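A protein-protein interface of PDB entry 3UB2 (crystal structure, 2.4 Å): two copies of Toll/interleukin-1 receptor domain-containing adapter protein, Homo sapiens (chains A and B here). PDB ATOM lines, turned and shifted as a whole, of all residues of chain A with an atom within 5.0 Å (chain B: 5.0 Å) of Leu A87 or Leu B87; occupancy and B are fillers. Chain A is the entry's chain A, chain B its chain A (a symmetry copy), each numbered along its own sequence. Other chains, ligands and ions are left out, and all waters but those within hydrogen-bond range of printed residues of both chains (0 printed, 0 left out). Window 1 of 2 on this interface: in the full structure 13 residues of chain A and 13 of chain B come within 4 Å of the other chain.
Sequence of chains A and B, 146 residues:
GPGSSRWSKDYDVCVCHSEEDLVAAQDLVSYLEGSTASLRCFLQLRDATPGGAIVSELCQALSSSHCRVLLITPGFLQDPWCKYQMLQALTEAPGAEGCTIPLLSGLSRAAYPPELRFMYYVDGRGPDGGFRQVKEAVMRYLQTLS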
ATOM      1  N   CYS A  82      24.671  18.058 -17.967  1.00  0.00           N
ATOM      2  CA  CYS A  82      26.039  18.356 -17.551  1.00  0.00           C
ATOM      3  C   CYS A  82      26.009  18.892 -16.124  1.00  0.00           C
ATOM      4  O   CYS A  82      26.768  18.436 -15.271  1.00  0.00           O
ATOM      5  CB  CYS A  82      26.673  19.412 -18.459  1.00  0.00           C
ATOM      6  SG  CYS A  82      26.986  18.866 -20.144  1.00  0.00           S
ATOM      7  N   LYS A  83      25.128  19.860 -15.876  1.00  0.00           N
ATOM      8  CA  LYS A  83      24.993  20.463 -14.553  1.00  0.00           C
ATOM      9  C   LYS A  83      24.608  19.438 -13.503  1.00  0.00           C
ATOM     10  O   LYS A  83      25.127  19.455 -12.386  1.00  0.00           O
ATOM     11  CB  LYS A  83      23.958  21.593 -14.577  1.00  0.00           C
ATOM     12  CG  LYS A  83      24.410  22.813 -15.364  1.00  0.00           C
ATOM     13  CD  LYS A  83      25.764  23.334 -14.874  1.00  0.00           C
ATOM     14  CE  LYS A  83      25.765  23.628 -13.377  1.00  0.00           C
ATOM     15  NZ  LYS A  83      24.829  24.728 -13.015  1.00  0.00           N
ATOM     16  N   TYR A  84      23.692  18.546 -13.856  1.00  0.00           N
ATOM     17  CA  TYR A  84      23.271  17.502 -12.936  1.00  0.00           C
ATOM     18  C   TYR A  84      24.454  16.565 -12.643  1.00  0.00           C
ATOM     19  O   TYR A  84      24.654  16.152 -11.502  1.00  0.00           O
ATOM     20  CB  TYR A  84      22.114  16.707 -13.536  1.00  0.00           C
ATOM     21  CG  TYR A  84      21.571  15.655 -12.605  1.00  0.00           C
ATOM     22  CD1 TYR A  84      20.868  16.014 -11.456  1.00  0.00           C
ATOM     23  CD2 TYR A  84      21.761  14.297 -12.866  1.00  0.00           C
ATOM     24  CE1 TYR A  84      20.363  15.047 -10.584  1.00  0.00           C
ATOM     25  CE2 TYR A  84      21.261  13.316 -12.001  1.00  0.00           C
ATOM     26  CZ  TYR A  84      20.563  13.701 -10.861  1.00  0.00           C
ATOM     27  OH  TYR A  84      20.083  12.744  -9.990  1.00  0.00           O
ATOM     28  N   GLN A  85      25.227  16.231 -13.678  1.00  0.00           N
ATOM     29  CA  GLN A  85      26.399  15.366 -13.524  1.00  0.00           C
ATOM     30  C   GLN A  85      27.439  16.039 -12.629  1.00  0.00           C
ATOM     31  O   GLN A  85      28.089  15.385 -11.813  1.00  0.00           O
ATOM     32  CB  GLN A  85      27.018  15.048 -14.893  1.00  0.00           C
ATOM     33  CG  GLN A  85      26.234  14.011 -15.686  1.00  0.00           C
ATOM     34  CD  GLN A  85      26.139  12.674 -14.964  1.00  0.00           C
ATOM     35  OE1 GLN A  85      27.151  12.017 -14.713  1.00  0.00           O
ATOM     36  NE2 GLN A  85      24.918  12.270 -14.624  1.00  0.00           N
ATOM     37  N   MET A  86      27.590  17.350 -12.794  1.00  0.00           N
ATOM     38  CA  MET A  86      28.522  18.121 -11.983  1.00  0.00           C
ATOM     39  C   MET A  86      28.068  18.014 -10.536  1.00  0.00           C
ATOM     40  O   MET A  86      28.876  17.854  -9.628  1.00  0.00           O
ATOM     41  CB  MET A  86      28.505  19.593 -12.402  1.00  0.00           C
ATOM     42  CG  MET A  86      29.286  20.510 -11.475  1.00  0.00           C
ATOM     43  SD  MET A  86      29.271  22.234 -12.015  1.00  0.00           S
ATOM     44  CE  MET A  86      28.563  23.046 -10.574  1.00  0.00           C
ATOM     45  N   LEU A  87      26.755  18.105 -10.341  1.00  0.00           N
ATOM     46  CA  LEU A  87      26.152  18.021  -9.021  1.00  0.00           C
ATOM     47  C   LEU A  87      26.448  16.665  -8.396  1.00  0.00           C
ATOM     48  O   LEU A  87      26.886  16.589  -7.251  1.00  0.00           O
ATOM     49  CB  LEU A  87      24.640  18.239  -9.132  1.00  0.00           C
ATOM     50  CG  LEU A  87      23.808  18.471  -7.871  1.00  0.00           C
ATOM     51  CD1 LEU A  87      23.612  17.167  -7.119  1.00  0.00           C
ATOM     52  CD2 LEU A  87      24.495  19.514  -7.003  1.00  0.00           C
ATOM     53  N   GLN A  88      26.210  15.596  -9.150  1.00  0.00           N
ATOM     54  CA  GLN A  88      26.463  14.253  -8.645  1.00  0.00           C
ATOM     55  C   GLN A  88      27.949  14.025  -8.452  1.00  0.00           C
ATOM     56  O   GLN A  88      28.357  13.314  -7.537  1.00  0.00           O
ATOM     57  CB  GLN A  88      25.900  13.194  -9.592  1.00  0.00           C
ATOM     58  CG  GLN A  88      24.392  13.077  -9.538  1.00  0.00           C
ATOM     59  CD  GLN A  88      23.899  11.719 -10.002  1.00  0.00           C
ATOM     60  OE1 GLN A  88      23.985  11.376 -11.183  1.00  0.00           O
ATOM     61  NE2 GLN A  88      23.385  10.932  -9.064  1.00  0.00           N
ATOM     62  N   ALA A  89      28.753  14.627  -9.323  1.00  0.00           N
ATOM     63  CA  ALA A  89      30.201  14.504  -9.222  1.00  0.00           C
ATOM     64  C   ALA A  89      30.643  15.064  -7.871  1.00  0.00           C
ATOM     65  O   ALA A  89      31.507  14.501  -7.212  1.00  0.00           O
ATOM     66  CB  ALA A  89      30.878  15.269 -10.359  1.00  0.00           C
ATOM     67  N   LEU A  90      30.032  16.174  -7.466  1.00  0.00           N
ATOM     68  CA  LEU A  90      30.349  16.816  -6.194  1.00  0.00           C
ATOM     69  C   LEU A  90      29.525  16.231  -5.048  1.00  0.00           C
ATOM     70  O   LEU A  90      29.820  16.477  -3.877  1.00  0.00           O
ATOM     71  CB  LEU A  90      30.094  18.317  -6.288  1.00  0.00           C
ATOM     72  CG  LEU A  90      30.933  19.056  -7.328  1.00  0.00           C
ATOM     73  CD1 LEU A  90      30.424  20.477  -7.482  1.00  0.00           C
ATOM     74  CD2 LEU A  90      32.392  19.036  -6.904  1.00  0.00           C
ATOM     75  N   THR A  91      28.488  15.467  -5.388  1.00  0.00           N
ATOM     76  CA  THR A  91      27.633  14.846  -4.376  1.00  0.00           C
ATOM     77  C   THR A  91      28.518  14.007  -3.470  1.00  0.00           C
ATOM     78  O   THR A  91      28.558  14.212  -2.260  1.00  0.00           O
ATOM     79  CB  THR A  91      26.550  13.934  -5.012  1.00  0.00           C
ATOM     80  OG1 THR A  91      25.440  14.736  -5.440  1.00  0.00           O
ATOM     81  CG2 THR A  91      26.061  12.886  -4.004  1.00  0.00           C
ATOM     82  N   MET A 119      35.398  26.817  -3.370  1.00  0.00           N
ATOM     83  CA  MET A 119      35.862  25.504  -3.784  1.00  0.00           C
ATOM     84  C   MET A 119      37.168  25.564  -4.560  1.00  0.00           C
ATOM     85  O   MET A 119      37.574  26.618  -5.055  1.00  0.00           O
ATOM     86  CB  MET A 119      34.805  24.837  -4.662  1.00  0.00           C
ATOM     87  CG  MET A 119      33.412  24.778  -4.051  1.00  0.00           C
ATOM     88  SD  MET A 119      32.175  24.358  -5.291  1.00  0.00           S
ATOM     89  CE  MET A 119      32.702  22.675  -5.678  1.00  0.00           C
ATOM     90  N   CYS B  82      25.448  31.108  -0.605  1.00  0.00           N
ATOM     91  CA  CYS B  82      24.144  30.470  -0.768  1.00  0.00           C
ATOM     92  C   CYS B  82      24.298  29.280  -1.709  1.00  0.00           C
ATOM     93  O   CYS B  82      23.833  28.183  -1.408  1.00  0.00           O
ATOM     94  CB  CYS B  82      23.127  31.442  -1.367  1.00  0.00           C
ATOM     95  SG  CYS B  82      22.660  32.803  -0.287  1.00  0.00           S
ATOM     96  N   LYS B  83      24.953  29.510  -2.846  1.00  0.00           N
ATOM     97  CA  LYS B  83      25.172  28.460  -3.838  1.00  0.00           C
ATOM     98  C   LYS B  83      25.970  27.303  -3.266  1.00  0.00           C
ATOM     99  O   LYS B  83      25.668  26.139  -3.530  1.00  0.00           O
ATOM    100  CB  LYS B  83      25.887  29.023  -5.071  1.00  0.00           C
ATOM    101  CG  LYS B  83      25.025  29.967  -5.893  1.00  0.00           C
ATOM    102  CD  LYS B  83      23.695  29.321  -6.291  1.00  0.00           C
ATOM    103  CE  LYS B  83      23.889  27.996  -7.021  1.00  0.00           C
ATOM    104  NZ  LYS B  83      24.585  28.166  -8.326  1.00  0.00           N
ATOM    105  N   TYR B  84      26.995  27.621  -2.486  1.00  0.00           N
ATOM    106  CA  TYR B  84      27.809  26.589  -1.864  1.00  0.00           C
ATOM    107  C   TYR B  84      26.955  25.790  -0.867  1.00  0.00           C
ATOM    108  O   TYR B  84      27.065  24.567  -0.792  1.00  0.00           O
ATOM    109  CB  TYR B  84      28.997  27.220  -1.142  1.00  0.00           C
ATOM    110  CG  TYR B  84      29.931  26.206  -0.538  1.00  0.00           C
ATOM    111  CD1 TYR B  84      30.721  25.391  -1.348  1.00  0.00           C
ATOM    112  CD2 TYR B  84      30.027  26.052   0.847  1.00  0.00           C
ATOM    113  CE1 TYR B  84      31.588  24.445  -0.798  1.00  0.00           C
ATOM    114  CE2 TYR B  84      30.892  25.108   1.413  1.00  0.00           C
ATOM    115  CZ  TYR B  84      31.669  24.308   0.582  1.00  0.00           C
ATOM    116  OH  TYR B  84      32.510  23.359   1.127  1.00  0.00           O
ATOM    117  N   GLN B  85      26.114  26.488  -0.102  1.00  0.00           N
ATOM    118  CA  GLN B  85      25.227  25.840   0.869  1.00  0.00           C
ATOM    119  C   GLN B  85      24.232  24.929   0.150  1.00  0.00           C
ATOM    120  O   GLN B  85      23.912  23.840   0.629  1.00  0.00           O
ATOM    121  CB  GLN B  85      24.470  26.891   1.692  1.00  0.00           C
ATOM    122  CG  GLN B  85      25.324  27.551   2.766  1.00  0.00           C
ATOM    123  CD  GLN B  85      25.863  26.551   3.780  1.00  0.00           C
ATOM    124  OE1 GLN B  85      25.097  25.905   4.498  1.00  0.00           O
ATOM    125  NE2 GLN B  85      27.185  26.419   3.839  1.00  0.00           N
ATOM    126  N   MET B  86      23.747  25.387  -1.000  1.00  0.00           N
ATOM    127  CA  MET B  86      22.817  24.605  -1.803  1.00  0.00           C
ATOM    128  C   MET B  86      23.532  23.332  -2.224  1.00  0.00           C
ATOM    129  O   MET B  86      22.959  22.248  -2.208  1.00  0.00           O
ATOM    130  CB  MET B  86      22.407  25.384  -3.056  1.00  0.00           C
ATOM    131  CG  MET B  86      21.607  24.568  -4.059  1.00  0.00           C
ATOM    132  SD  MET B  86      21.115  25.524  -5.510  1.00  0.00           S
ATOM    133  CE  MET B  86      21.853  24.554  -6.834  1.00  0.00           C
ATOM    134  N   LEU B  87      24.799  23.486  -2.602  1.00  0.00           N
ATOM    135  CA  LEU B  87      25.628  22.373  -3.032  1.00  0.00           C
ATOM    136  C   LEU B  87      25.779  21.366  -1.900  1.00  0.00           C
ATOM    137  O   LEU B  87      25.582  20.170  -2.101  1.00  0.00           O
ATOM    138  CB  LEU B  87      27.000  22.894  -3.469  1.00  0.00           C
ATOM    139  CG  LEU B  87      27.963  21.972  -4.219  1.00  0.00           C
ATOM    140  CD1 LEU B  87      28.594  20.977  -3.261  1.00  0.00           C
ATOM    141  CD2 LEU B  87      27.212  21.267  -5.337  1.00  0.00           C
ATOM    142  N   GLN B  88      26.128  21.851  -0.713  1.00  0.00           N
ATOM    143  CA  GLN B  88      26.296  20.970   0.435  1.00  0.00           C
ATOM    144  C   GLN B  88      24.966  20.375   0.853  1.00  0.00           C
ATOM    145  O   GLN B  88      24.908  19.237   1.313  1.00  0.00           O
ATOM    146  CB  GLN B  88      26.918  21.716   1.615  1.00  0.00           C
ATOM    147  CG  GLN B  88      28.396  21.994   1.441  1.00  0.00           C
ATOM    148  CD  GLN B  88      29.108  22.193   2.766  1.00  0.00           C
ATOM    149  OE1 GLN B  88      28.899  23.189   3.462  1.00  0.00           O
ATOM    150  NE2 GLN B  88      29.953  21.234   3.126  1.00  0.00           N
ATOM    151  N   ALA B  89      23.900  21.155   0.698  1.00  0.00           N
ATOM    152  CA  ALA B  89      22.565  20.683   1.039  1.00  0.00           C
ATOM    153  C   ALA B  89      22.249  19.459   0.181  1.00  0.00           C
ATOM    154  O   ALA B  89      21.675  18.490   0.661  1.00  0.00           O
ATOM    155  CB  ALA B  89      21.534  21.784   0.789  1.00  0.00           C
ATOM    156  N   LEU B  90      22.639  19.513  -1.089  1.00  0.00           N
ATOM    157  CA  LEU B  90      22.409  18.414  -2.021  1.00  0.00           C
ATOM    158  C   LEU B  90      23.539  17.386  -1.969  1.00  0.00           C
ATOM    159  O   LEU B  90      23.406  16.284  -2.503  1.00  0.00           O
ATOM    160  CB  LEU B  90      22.278  18.952  -3.442  1.00  0.00           C
ATOM    161  CG  LEU B  90      21.116  19.917  -3.668  1.00  0.00           C
ATOM    162  CD1 LEU B  90      21.236  20.551  -5.042  1.00  0.00           C
ATOM    163  CD2 LEU B  90      19.803  19.167  -3.521  1.00  0.00           C
ATOM    164  N   THR B  91      24.650  17.753  -1.333  1.00  0.00           N
ATOM    165  CA  THR B  91      25.794  16.849  -1.212  1.00  0.00           C
ATOM    166  C   THR B  91      25.309  15.573  -0.545  1.00  0.00           C
ATOM    167  O   THR B  91      25.437  14.484  -1.099  1.00  0.00           O
ATOM    168  CB  THR B  91      26.933  17.466  -0.357  1.00  0.00           C
ATOM    169  OG1 THR B  91      27.725  18.339  -1.173  1.00  0.00           O
ATOM    170  CG2 THR B  91      27.829  16.368   0.230  1.00  0.00           C
ATOM    171  N   MET B 119      15.704  17.161 -11.346  1.00  0.00           N
ATOM    172  CA  MET B 119      15.500  17.097  -9.908  1.00  0.00           C
ATOM    173  C   MET B 119      14.102  17.528  -9.497  1.00  0.00           C
ATOM    174  O   MET B 119      13.374  18.167 -10.261  1.00  0.00           O
ATOM    175  CB  MET B 119      16.513  17.998  -9.204  1.00  0.00           C
ATOM    176  CG  MET B 119      17.965  17.743  -9.582  1.00  0.00           C
ATOM    177  SD  MET B 119      19.027  19.089  -9.030  1.00  0.00           S
ATOM    178  CE  MET B 119      18.856  18.890  -7.244  1.00  0.00           C
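O of Thr B91 sits close to O of Thr A91 (3.3 Å).
The backbone carbonyl oxygen (O) of Leu B87 is in hydrogen-bond range of the side-chain hydroxyl (OG1) of Thr B91, at 3.0 Å.
The backbone carbonyl oxygen of Leu A87 sits at hydrogen-bond distance from the side-chain hydroxyl of Thr A91.
CG of Met B119 touches CE1 of Tyr A84 (3.7 Å).
Leu A87 touches Leu B87 (CD2 to CD2, 3.6 Å).
CD1 of Leu B90 touches CD2 of Leu A87, at 3.9 Å.
CD2 of Leu B87 touches CD1 of Leu A90 (3.9 Å).
Thr B91 touches Leu A90.
Thr A91 touches Leu B90 (OG1 to O, 3.9 Å).
Met A119 touches Tyr B84 (CG to CE1, 3.7 Å).
Of the printed residues of chain B, Leu A87 touches Leu B87 (3.6 Å) and Leu B90 (3.9 Å).
Of the printed residues of chain A, Tyr B84 touches Met A119.
Met B86 touches none of the printed residues of chain A.
Of chain A, only Leu A87 (3.6 Å) and Leu A90 (3.9 Å) come within 4 Å of Leu B87.
Ala B89 touches none of the printed residues of chain A.
Printed residues of chain A within 4 Å of Met B119: Tyr A84.
Hydrophobic or aromatic side chains of chain B within 4 Å of the printed part of chain A: Tyr B84, Leu B87, Leu B90 and Met B119.
Printed residues of chain A that touch a printed residue of chain B: Tyr A84, Leu A87, Leu A90, Thr A91 and Met A119.
Hydrophobic or aromatic side chains of chain A within 4 Å of the printed part of chain B: Tyr A84, Leu A87, Leu A90 and Met A119.
Tyr A84 touches Met B119, and with the chains exchanged Met A119 touches Tyr B84.
Leu B87 touches its own counterpart, Leu A87.
Leu A87 touches Leu B90, and with the chains exchanged Leu A90 touches Leu B87.
Leu A90 touches Thr B91, and with the chains exchanged Thr A91 touches Leu B90.
Positions printed for both chains: 82, 83, 84, 85, 86, 87, 88, 89, 90, 91 and 119.
Of the 8 pairs that touch across the chains among the printed residues, 8 have their exchanged pair printed and touching as well.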
